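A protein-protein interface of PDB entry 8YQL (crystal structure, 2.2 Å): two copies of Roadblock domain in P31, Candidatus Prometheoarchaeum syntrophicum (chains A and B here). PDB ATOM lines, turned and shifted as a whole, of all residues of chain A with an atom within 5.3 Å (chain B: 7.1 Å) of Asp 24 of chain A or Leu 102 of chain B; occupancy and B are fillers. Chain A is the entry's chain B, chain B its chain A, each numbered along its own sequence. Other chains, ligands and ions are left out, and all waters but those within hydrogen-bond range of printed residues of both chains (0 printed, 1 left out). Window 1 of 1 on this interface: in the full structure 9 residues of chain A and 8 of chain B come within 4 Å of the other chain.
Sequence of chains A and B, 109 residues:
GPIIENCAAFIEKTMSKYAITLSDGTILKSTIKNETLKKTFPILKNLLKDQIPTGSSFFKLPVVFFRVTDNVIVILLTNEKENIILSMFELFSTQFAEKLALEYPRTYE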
ATOM      1  N   LEU A  22      -5.803  33.351  -8.332  1.00  0.00           N
ATOM      2  CA  LEU A  22      -5.462  32.009  -7.907  1.00  0.00           C
ATOM      3  C   LEU A  22      -4.731  31.294  -9.034  1.00  0.00           C
ATOM      4  O   LEU A  22      -4.805  31.685 -10.204  1.00  0.00           O
ATOM      5  CB  LEU A  22      -6.723  31.243  -7.495  1.00  0.00           C
ATOM      6  CG  LEU A  22      -7.456  31.878  -6.318  1.00  0.00           C
ATOM      7  CD1 LEU A  22      -8.509  30.918  -5.783  1.00  0.00           C
ATOM      8  CD2 LEU A  22      -6.474  32.229  -5.207  1.00  0.00           C
ATOM      9  N   SER A  23      -4.031  30.217  -8.674  1.00  0.00           N
ATOM     10  CA  SER A  23      -3.272  29.485  -9.665  1.00  0.00           C
ATOM     11  C   SER A  23      -4.163  28.650 -10.571  1.00  0.00           C
ATOM     12  O   SER A  23      -3.647  28.047 -11.520  1.00  0.00           O
ATOM     13  CB  SER A  23      -2.228  28.600  -8.987  1.00  0.00           C
ATOM     14  OG  SER A  23      -2.877  27.689  -8.127  1.00  0.00           O
ATOM     15  N   ASP A  24      -5.476  28.599 -10.321  1.00  0.00           N
ATOM     16  CA  ASP A  24      -6.391  28.000 -11.292  1.00  0.00           C
ATOM     17  C   ASP A  24      -7.039  29.040 -12.198  1.00  0.00           C
ATOM     18  O   ASP A  24      -7.836  28.671 -13.066  1.00  0.00           O
ATOM     19  CB  ASP A  24      -7.468  27.146 -10.593  1.00  0.00           C
ATOM     20  CG  ASP A  24      -8.405  27.963  -9.699  1.00  0.00           C
ATOM     21  OD1 ASP A  24      -8.404  29.211  -9.755  1.00  0.00           O
ATOM     22  OD2 ASP A  24      -9.130  27.345  -8.893  1.00  0.00           O
ATOM     23  N   GLY A  25      -6.709  30.325 -12.014  1.00  0.00           N
ATOM     24  CA  GLY A  25      -7.130  31.389 -12.906  1.00  0.00           C
ATOM     25  C   GLY A  25      -8.170  32.310 -12.329  1.00  0.00           C
ATOM     26  O   GLY A  25      -8.468  33.335 -12.949  1.00  0.00           O
ATOM     27  N   THR A  26      -8.714  32.000 -11.150  1.00  0.00           N
ATOM     28  CA  THR A  26      -9.723  32.853 -10.529  1.00  0.00           C
ATOM     29  C   THR A  26      -9.136  34.235 -10.282  1.00  0.00           C
ATOM     30  O   THR A  26      -8.088  34.357  -9.650  1.00  0.00           O
ATOM     31  CB  THR A  26     -10.189  32.231  -9.203  1.00  0.00           C
ATOM     32  OG1 THR A  26     -10.575  30.876  -9.417  1.00  0.00           O
ATOM     33  CG2 THR A  26     -11.360  32.984  -8.624  1.00  0.00           C
ATOM     34  N   PHE A  41      -2.409  34.739 -19.796  1.00  0.00           N
ATOM     35  CA  PHE A  41      -2.569  33.395 -19.236  1.00  0.00           C
ATOM     36  C   PHE A  41      -1.767  32.297 -19.943  1.00  0.00           C
ATOM     37  O   PHE A  41      -1.309  31.384 -19.238  1.00  0.00           O
ATOM     38  CB  PHE A  41      -4.067  33.031 -19.207  1.00  0.00           C
ATOM     39  CG  PHE A  41      -4.819  33.639 -18.037  1.00  0.00           C
ATOM     40  CD1 PHE A  41      -4.183  34.499 -17.156  1.00  0.00           C
ATOM     41  CD2 PHE A  41      -6.150  33.324 -17.806  1.00  0.00           C
ATOM     42  CE1 PHE A  41      -4.866  35.039 -16.079  1.00  0.00           C
ATOM     43  CE2 PHE A  41      -6.843  33.858 -16.721  1.00  0.00           C
ATOM     44  CZ  PHE A  41      -6.205  34.714 -15.861  1.00  0.00           C
ATOM     45  N   LEU A  44       1.405  32.356 -18.040  1.00  0.00           N
ATOM     46  CA  LEU A  44       1.185  31.840 -16.695  1.00  0.00           C
ATOM     47  C   LEU A  44       1.048  30.331 -16.728  1.00  0.00           C
ATOM     48  O   LEU A  44       1.691  29.624 -15.943  1.00  0.00           O
ATOM     49  CB  LEU A  44      -0.056  32.477 -16.071  1.00  0.00           C
ATOM     50  CG  LEU A  44      -0.455  31.975 -14.688  1.00  0.00           C
ATOM     51  CD1 LEU A  44       0.743  31.922 -13.771  1.00  0.00           C
ATOM     52  CD2 LEU A  44      -1.488  32.925 -14.116  1.00  0.00           C
ATOM     53  N   LYS A  45       0.245  29.816 -17.663  1.00  0.00           N
ATOM     54  CA  LYS A  45       0.055  28.370 -17.743  1.00  0.00           C
ATOM     55  C   LYS A  45       1.385  27.651 -17.890  1.00  0.00           C
ATOM     56  O   LYS A  45       1.630  26.644 -17.220  1.00  0.00           O
ATOM     57  CB  LYS A  45      -0.869  28.022 -18.904  1.00  0.00           C
ATOM     58  CG  LYS A  45      -1.221  26.542 -19.002  1.00  0.00           C
ATOM     59  CD  LYS A  45      -1.638  26.178 -20.423  1.00  0.00           C
ATOM     60  CE  LYS A  45      -2.125  24.748 -20.504  1.00  0.00           C
ATOM     61  NZ  LYS A  45      -2.550  24.281 -19.140  1.00  0.00           N
ATOM     62  N   LEU A  48       3.300  27.678 -14.507  1.00  0.00           N
ATOM     63  CA  LEU A  48       2.765  26.741 -13.527  1.00  0.00           C
ATOM     64  C   LEU A  48       3.077  25.302 -13.915  1.00  0.00           C
ATOM     65  O   LEU A  48       3.331  24.466 -13.045  1.00  0.00           O
ATOM     66  CB  LEU A  48       1.256  26.942 -13.374  1.00  0.00           C
ATOM     67  CG  LEU A  48       0.845  28.242 -12.687  1.00  0.00           C
ATOM     68  CD1 LEU A  48      -0.672  28.374 -12.696  1.00  0.00           C
ATOM     69  CD2 LEU A  48       1.368  28.283 -11.257  1.00  0.00           C
ATOM     70  N   ASN A  71      -0.783  28.848  -4.421  1.00  0.00           N
ATOM     71  CA  ASN A  71      -2.070  29.079  -5.060  1.00  0.00           C
ATOM     72  C   ASN A  71      -2.380  30.552  -5.339  1.00  0.00           C
ATOM     73  O   ASN A  71      -3.502  30.861  -5.750  1.00  0.00           O
ATOM     74  CB  ASN A  71      -3.180  28.477  -4.190  1.00  0.00           C
ATOM     75  CG  ASN A  71      -4.491  28.320  -4.947  1.00  0.00           C
ATOM     76  OD1 ASN A  71      -4.504  27.842  -6.082  1.00  0.00           O
ATOM     77  ND2 ASN A  71      -5.598  28.714  -4.320  1.00  0.00           N
ATOM     78  N   THR A 107      -6.979  24.046  -4.036  1.00  0.00           N
ATOM     79  CA  THR A 107      -8.046  23.060  -3.961  1.00  0.00           C
ATOM     80  C   THR A 107      -8.167  22.303  -5.273  1.00  0.00           C
ATOM     81  O   THR A 107      -8.001  22.878  -6.351  1.00  0.00           O
ATOM     82  CB  THR A 107      -9.378  23.704  -3.595  1.00  0.00           C
ATOM     83  OG1 THR A 107     -10.211  22.709  -3.001  1.00  0.00           O
ATOM     84  CG2 THR A 107     -10.076  24.293  -4.812  1.00  0.00           C
ATOM     85  N   THR B  69     -15.163  31.066 -23.420  1.00  0.00           N
ATOM     86  CA  THR B  69     -13.954  31.866 -23.462  1.00  0.00           C
ATOM     87  C   THR B  69     -13.527  32.004 -24.906  1.00  0.00           C
ATOM     88  O   THR B  69     -14.114  31.409 -25.815  1.00  0.00           O
ATOM     89  CB  THR B  69     -12.818  31.246 -22.649  1.00  0.00           C
ATOM     90  OG1 THR B  69     -12.376  30.059 -23.320  1.00  0.00           O
ATOM     91  CG2 THR B  69     -13.282  30.905 -21.250  1.00  0.00           C
ATOM     92  N   PHE B  96     -16.926  28.476 -14.224  1.00  0.00           N
ATOM     93  CA  PHE B  96     -15.843  27.836 -14.977  1.00  0.00           C
ATOM     94  C   PHE B  96     -15.033  28.731 -15.909  1.00  0.00           C
ATOM     95  O   PHE B  96     -13.958  28.291 -16.336  1.00  0.00           O
ATOM     96  CB  PHE B  96     -16.378  26.659 -15.815  1.00  0.00           C
ATOM     97  CG  PHE B  96     -16.914  25.519 -14.989  1.00  0.00           C
ATOM     98  CD1 PHE B  96     -16.060  24.741 -14.224  1.00  0.00           C
ATOM     99  CD2 PHE B  96     -18.257  25.203 -15.003  1.00  0.00           C
ATOM    100  CE1 PHE B  96     -16.547  23.689 -13.464  1.00  0.00           C
ATOM    101  CE2 PHE B  96     -18.755  24.158 -14.239  1.00  0.00           C
ATOM    102  CZ  PHE B  96     -17.905  23.398 -13.471  1.00  0.00           C
ATOM    103  N   ALA B  97     -15.487  29.943 -16.250  1.00  0.00           N
ATOM    104  CA  ALA B  97     -14.858  30.687 -17.341  1.00  0.00           C
ATOM    105  C   ALA B  97     -13.422  31.095 -17.024  1.00  0.00           C
ATOM    106  O   ALA B  97     -12.543  30.982 -17.886  1.00  0.00           O
ATOM    107  CB  ALA B  97     -15.673  31.924 -17.701  1.00  0.00           C
ATOM    108  N   GLU B  98     -13.155  31.592 -15.816  1.00  0.00           N
ATOM    109  CA  GLU B  98     -11.780  31.990 -15.523  1.00  0.00           C
ATOM    110  C   GLU B  98     -10.862  30.775 -15.449  1.00  0.00           C
ATOM    111  O   GLU B  98      -9.743  30.794 -15.986  1.00  0.00           O
ATOM    112  CB  GLU B  98     -11.733  32.807 -14.241  1.00  0.00           C
ATOM    113  CG  GLU B  98     -12.297  34.201 -14.461  1.00  0.00           C
ATOM    114  CD  GLU B  98     -12.459  34.996 -13.180  1.00  0.00           C
ATOM    115  OE1 GLU B  98     -12.155  34.463 -12.092  1.00  0.00           O
ATOM    116  OE2 GLU B  98     -12.873  36.174 -13.265  1.00  0.00           O
ATOM    117  N   LYS B  99     -11.335  29.688 -14.848  1.00  0.00           N
ATOM    118  CA  LYS B  99     -10.553  28.459 -14.873  1.00  0.00           C
ATOM    119  C   LYS B  99     -10.305  27.988 -16.302  1.00  0.00           C
ATOM    120  O   LYS B  99      -9.167  27.706 -16.689  1.00  0.00           O
ATOM    121  CB  LYS B  99     -11.264  27.393 -14.049  1.00  0.00           C
ATOM    122  CG  LYS B  99     -11.052  27.598 -12.561  1.00  0.00           C
ATOM    123  CD  LYS B  99     -11.562  26.421 -11.773  1.00  0.00           C
ATOM    124  CE  LYS B  99     -13.021  26.585 -11.410  1.00  0.00           C
ATOM    125  NZ  LYS B  99     -13.217  26.378  -9.946  1.00  0.00           N
ATOM    126  N   LEU B 100     -11.359  27.907 -17.110  1.00  0.00           N
ATOM    127  CA  LEU B 100     -11.193  27.437 -18.480  1.00  0.00           C
ATOM    128  C   LEU B 100     -10.234  28.334 -19.257  1.00  0.00           C
ATOM    129  O   LEU B 100      -9.417  27.846 -20.050  1.00  0.00           O
ATOM    130  CB  LEU B 100     -12.556  27.376 -19.180  1.00  0.00           C
ATOM    131  CG  LEU B 100     -13.448  26.196 -18.807  1.00  0.00           C
ATOM    132  CD1 LEU B 100     -14.760  26.339 -19.530  1.00  0.00           C
ATOM    133  CD2 LEU B 100     -12.786  24.843 -19.128  1.00  0.00           C
ATOM    134  N   ALA B 101     -10.320  29.648 -19.040  1.00  0.00           N
ATOM    135  CA  ALA B 101      -9.419  30.578 -19.720  1.00  0.00           C
ATOM    136  C   ALA B 101      -7.948  30.272 -19.419  1.00  0.00           C
ATOM    137  O   ALA B 101      -7.091  30.429 -20.299  1.00  0.00           O
ATOM    138  CB  ALA B 101      -9.766  32.017 -19.324  1.00  0.00           C
ATOM    139  N   LEU B 102      -7.633  29.856 -18.182  1.00  0.00           N
ATOM    140  CA  LEU B 102      -6.250  29.501 -17.837  1.00  0.00           C
ATOM    141  C   LEU B 102      -5.873  28.107 -18.333  1.00  0.00           C
ATOM    142  O   LEU B 102      -4.747  27.891 -18.798  1.00  0.00           O
ATOM    143  CB  LEU B 102      -6.021  29.575 -16.323  1.00  0.00           C
ATOM    144  CG  LEU B 102      -4.623  29.044 -15.938  1.00  0.00           C
ATOM    145  CD1 LEU B 102      -3.514  29.891 -16.594  1.00  0.00           C
ATOM    146  CD2 LEU B 102      -4.385  28.954 -14.451  1.00  0.00           C
ATOM    147  N   GLU B 103      -6.789  27.144 -18.234  1.00  0.00           N
ATOM    148  CA  GLU B 103      -6.471  25.777 -18.646  1.00  0.00           C
ATOM    149  C   GLU B 103      -6.289  25.649 -20.157  1.00  0.00           C
ATOM    150  O   GLU B 103      -5.445  24.862 -20.606  1.00  0.00           O
ATOM    151  CB  GLU B 103      -7.570  24.832 -18.160  1.00  0.00           C
ATOM    152  CG  GLU B 103      -7.196  23.331 -18.166  1.00  0.00           C
ATOM    153  CD  GLU B 103      -5.891  23.034 -17.428  1.00  0.00           C
ATOM    154  OE1 GLU B 103      -5.047  22.275 -17.969  1.00  0.00           O
ATOM    155  OE2 GLU B 103      -5.708  23.569 -16.312  1.00  0.00           O
ATOM    156  N   TYR B 104      -7.045  26.414 -20.954  1.00  0.00           N
ATOM    157  CA  TYR B 104      -7.025  26.308 -22.417  1.00  0.00           C
ATOM    158  C   TYR B 104      -6.838  27.675 -23.077  1.00  0.00           C
ATOM    159  O   TYR B 104      -7.719  28.158 -23.793  1.00  0.00           O
ATOM    160  CB  TYR B 104      -8.315  25.642 -22.906  1.00  0.00           C
ATOM    161  CG  TYR B 104      -8.564  24.282 -22.285  1.00  0.00           C
ATOM    162  CD1 TYR B 104      -7.898  23.159 -22.752  1.00  0.00           C
ATOM    163  CD2 TYR B 104      -9.447  24.127 -21.211  1.00  0.00           C
ATOM    164  CE1 TYR B 104      -8.108  21.905 -22.176  1.00  0.00           C
ATOM    165  CE2 TYR B 104      -9.666  22.891 -20.632  1.00  0.00           C
ATOM    166  CZ  TYR B 104      -8.990  21.779 -21.118  1.00  0.00           C
ATOM    167  OH  TYR B 104      -9.184  20.537 -20.548  1.00  0.00           O
ATOM    168  N   PRO B 105      -5.699  28.336 -22.855  1.00  0.00           N
ATOM    169  CA  PRO B 105      -5.523  29.683 -23.424  1.00  0.00           C
ATOM    170  C   PRO B 105      -5.345  29.643 -24.936  1.00  0.00           C
ATOM    171  O   PRO B 105      -4.675  28.760 -25.480  1.00  0.00           O
ATOM    172  CB  PRO B 105      -4.250  30.210 -22.745  1.00  0.00           C
ATOM    173  CG  PRO B 105      -3.830  29.175 -21.757  1.00  0.00           C
ATOM    174  CD  PRO B 105      -4.513  27.886 -22.102  1.00  0.00           C
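The side-chain carboxylate (OE1) of Glu 103 of chain B is in salt-bridge range of the side-chain amino group (NZ) of Lys 45 of chain A (3.4 Å).
The side-chain hydroxyl (OG) of Ser 23 of chain A sits at hydrogen-bond distance from the side-chain amide oxygen (OD1) of Asn 71 of chain A, at 2.6 Å.
The side-chain hydroxyl (OG1) of Thr 26 of chain A is in hydrogen-bond range of the side-chain carboxylate (OD1) of Asp 24 of chain A (2.8 Å).
Among the printed residues, merely in contact across the chains: Ser 23 of chain A with Leu 102 of chain B (3.2 Å), Asp 24 of chain A with Lys 99 of chain B (3.3 Å), Thr 26 of chain A with Glu 98 of chain B (3.3 Å), Asp 24 of chain A with Leu 102 of chain B (3.5 Å), Gly 25 of chain A with Glu 98 of chain B (3.6 Å), Gly 25 of chain A with Leu 102 of chain B (3.6 Å), Lys 45 of chain A with Pro 105 of chain B (3.7 Å), Phe 41 of chain A with Leu 102 of chain B (3.8 Å), Lys 45 of chain A with Leu 102 of chain B (3.8 Å) and Phe 41 of chain A with Ala 101 of chain B (3.9 Å).
Asp 24 of chain A touches just these residues of chain B: Lys 99 (3.3 Å) and Leu 102 (3.5 Å).
Of the printed residues of chain B, Phe 41 of chain A touches Ala 101 and Leu 102.
Of the printed residues of chain A, Pro 105 of chain B touches Lys 45.
The nearest residue of chain B that does not touch Asp 24 of chain A is Glu 98 of chain B (4.1 Å).
The nearest printed residue of chain A that does not touch Leu 102 of chain B is Leu 48 of chain A (4.1 Å).
The nearest printed residue of chain A that does not touch Glu 98 of chain B is Asp 24 of chain A (4.1 Å).
Of the 11 printed residues of chain B, 6 touch a printed residue of chain A.
Hydrophobic or aromatic side chains of chain B that line the printed part of chain A: Leu 102 and Pro 105.
Printed residues of chain A that touch a printed residue of chain B: Ser 23, Asp 24, Gly 25, Thr 26, Phe 41 and Lys 45.
Along chain A the printed residues that touch a printed residue of chain B span positions 23 to 45.
Among the printed residues, Asp or Glu carboxylates within 4 Å of a Lys or Arg side-chain nitrogen of the other chain: Lys 45 of chain A with Glu 103 of chain B (3.4 Å).
No position is printed for both chains.
Of the 11 pairs that touch across the chains among the printed residues, none has its exchanged pair printed and touching as well.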
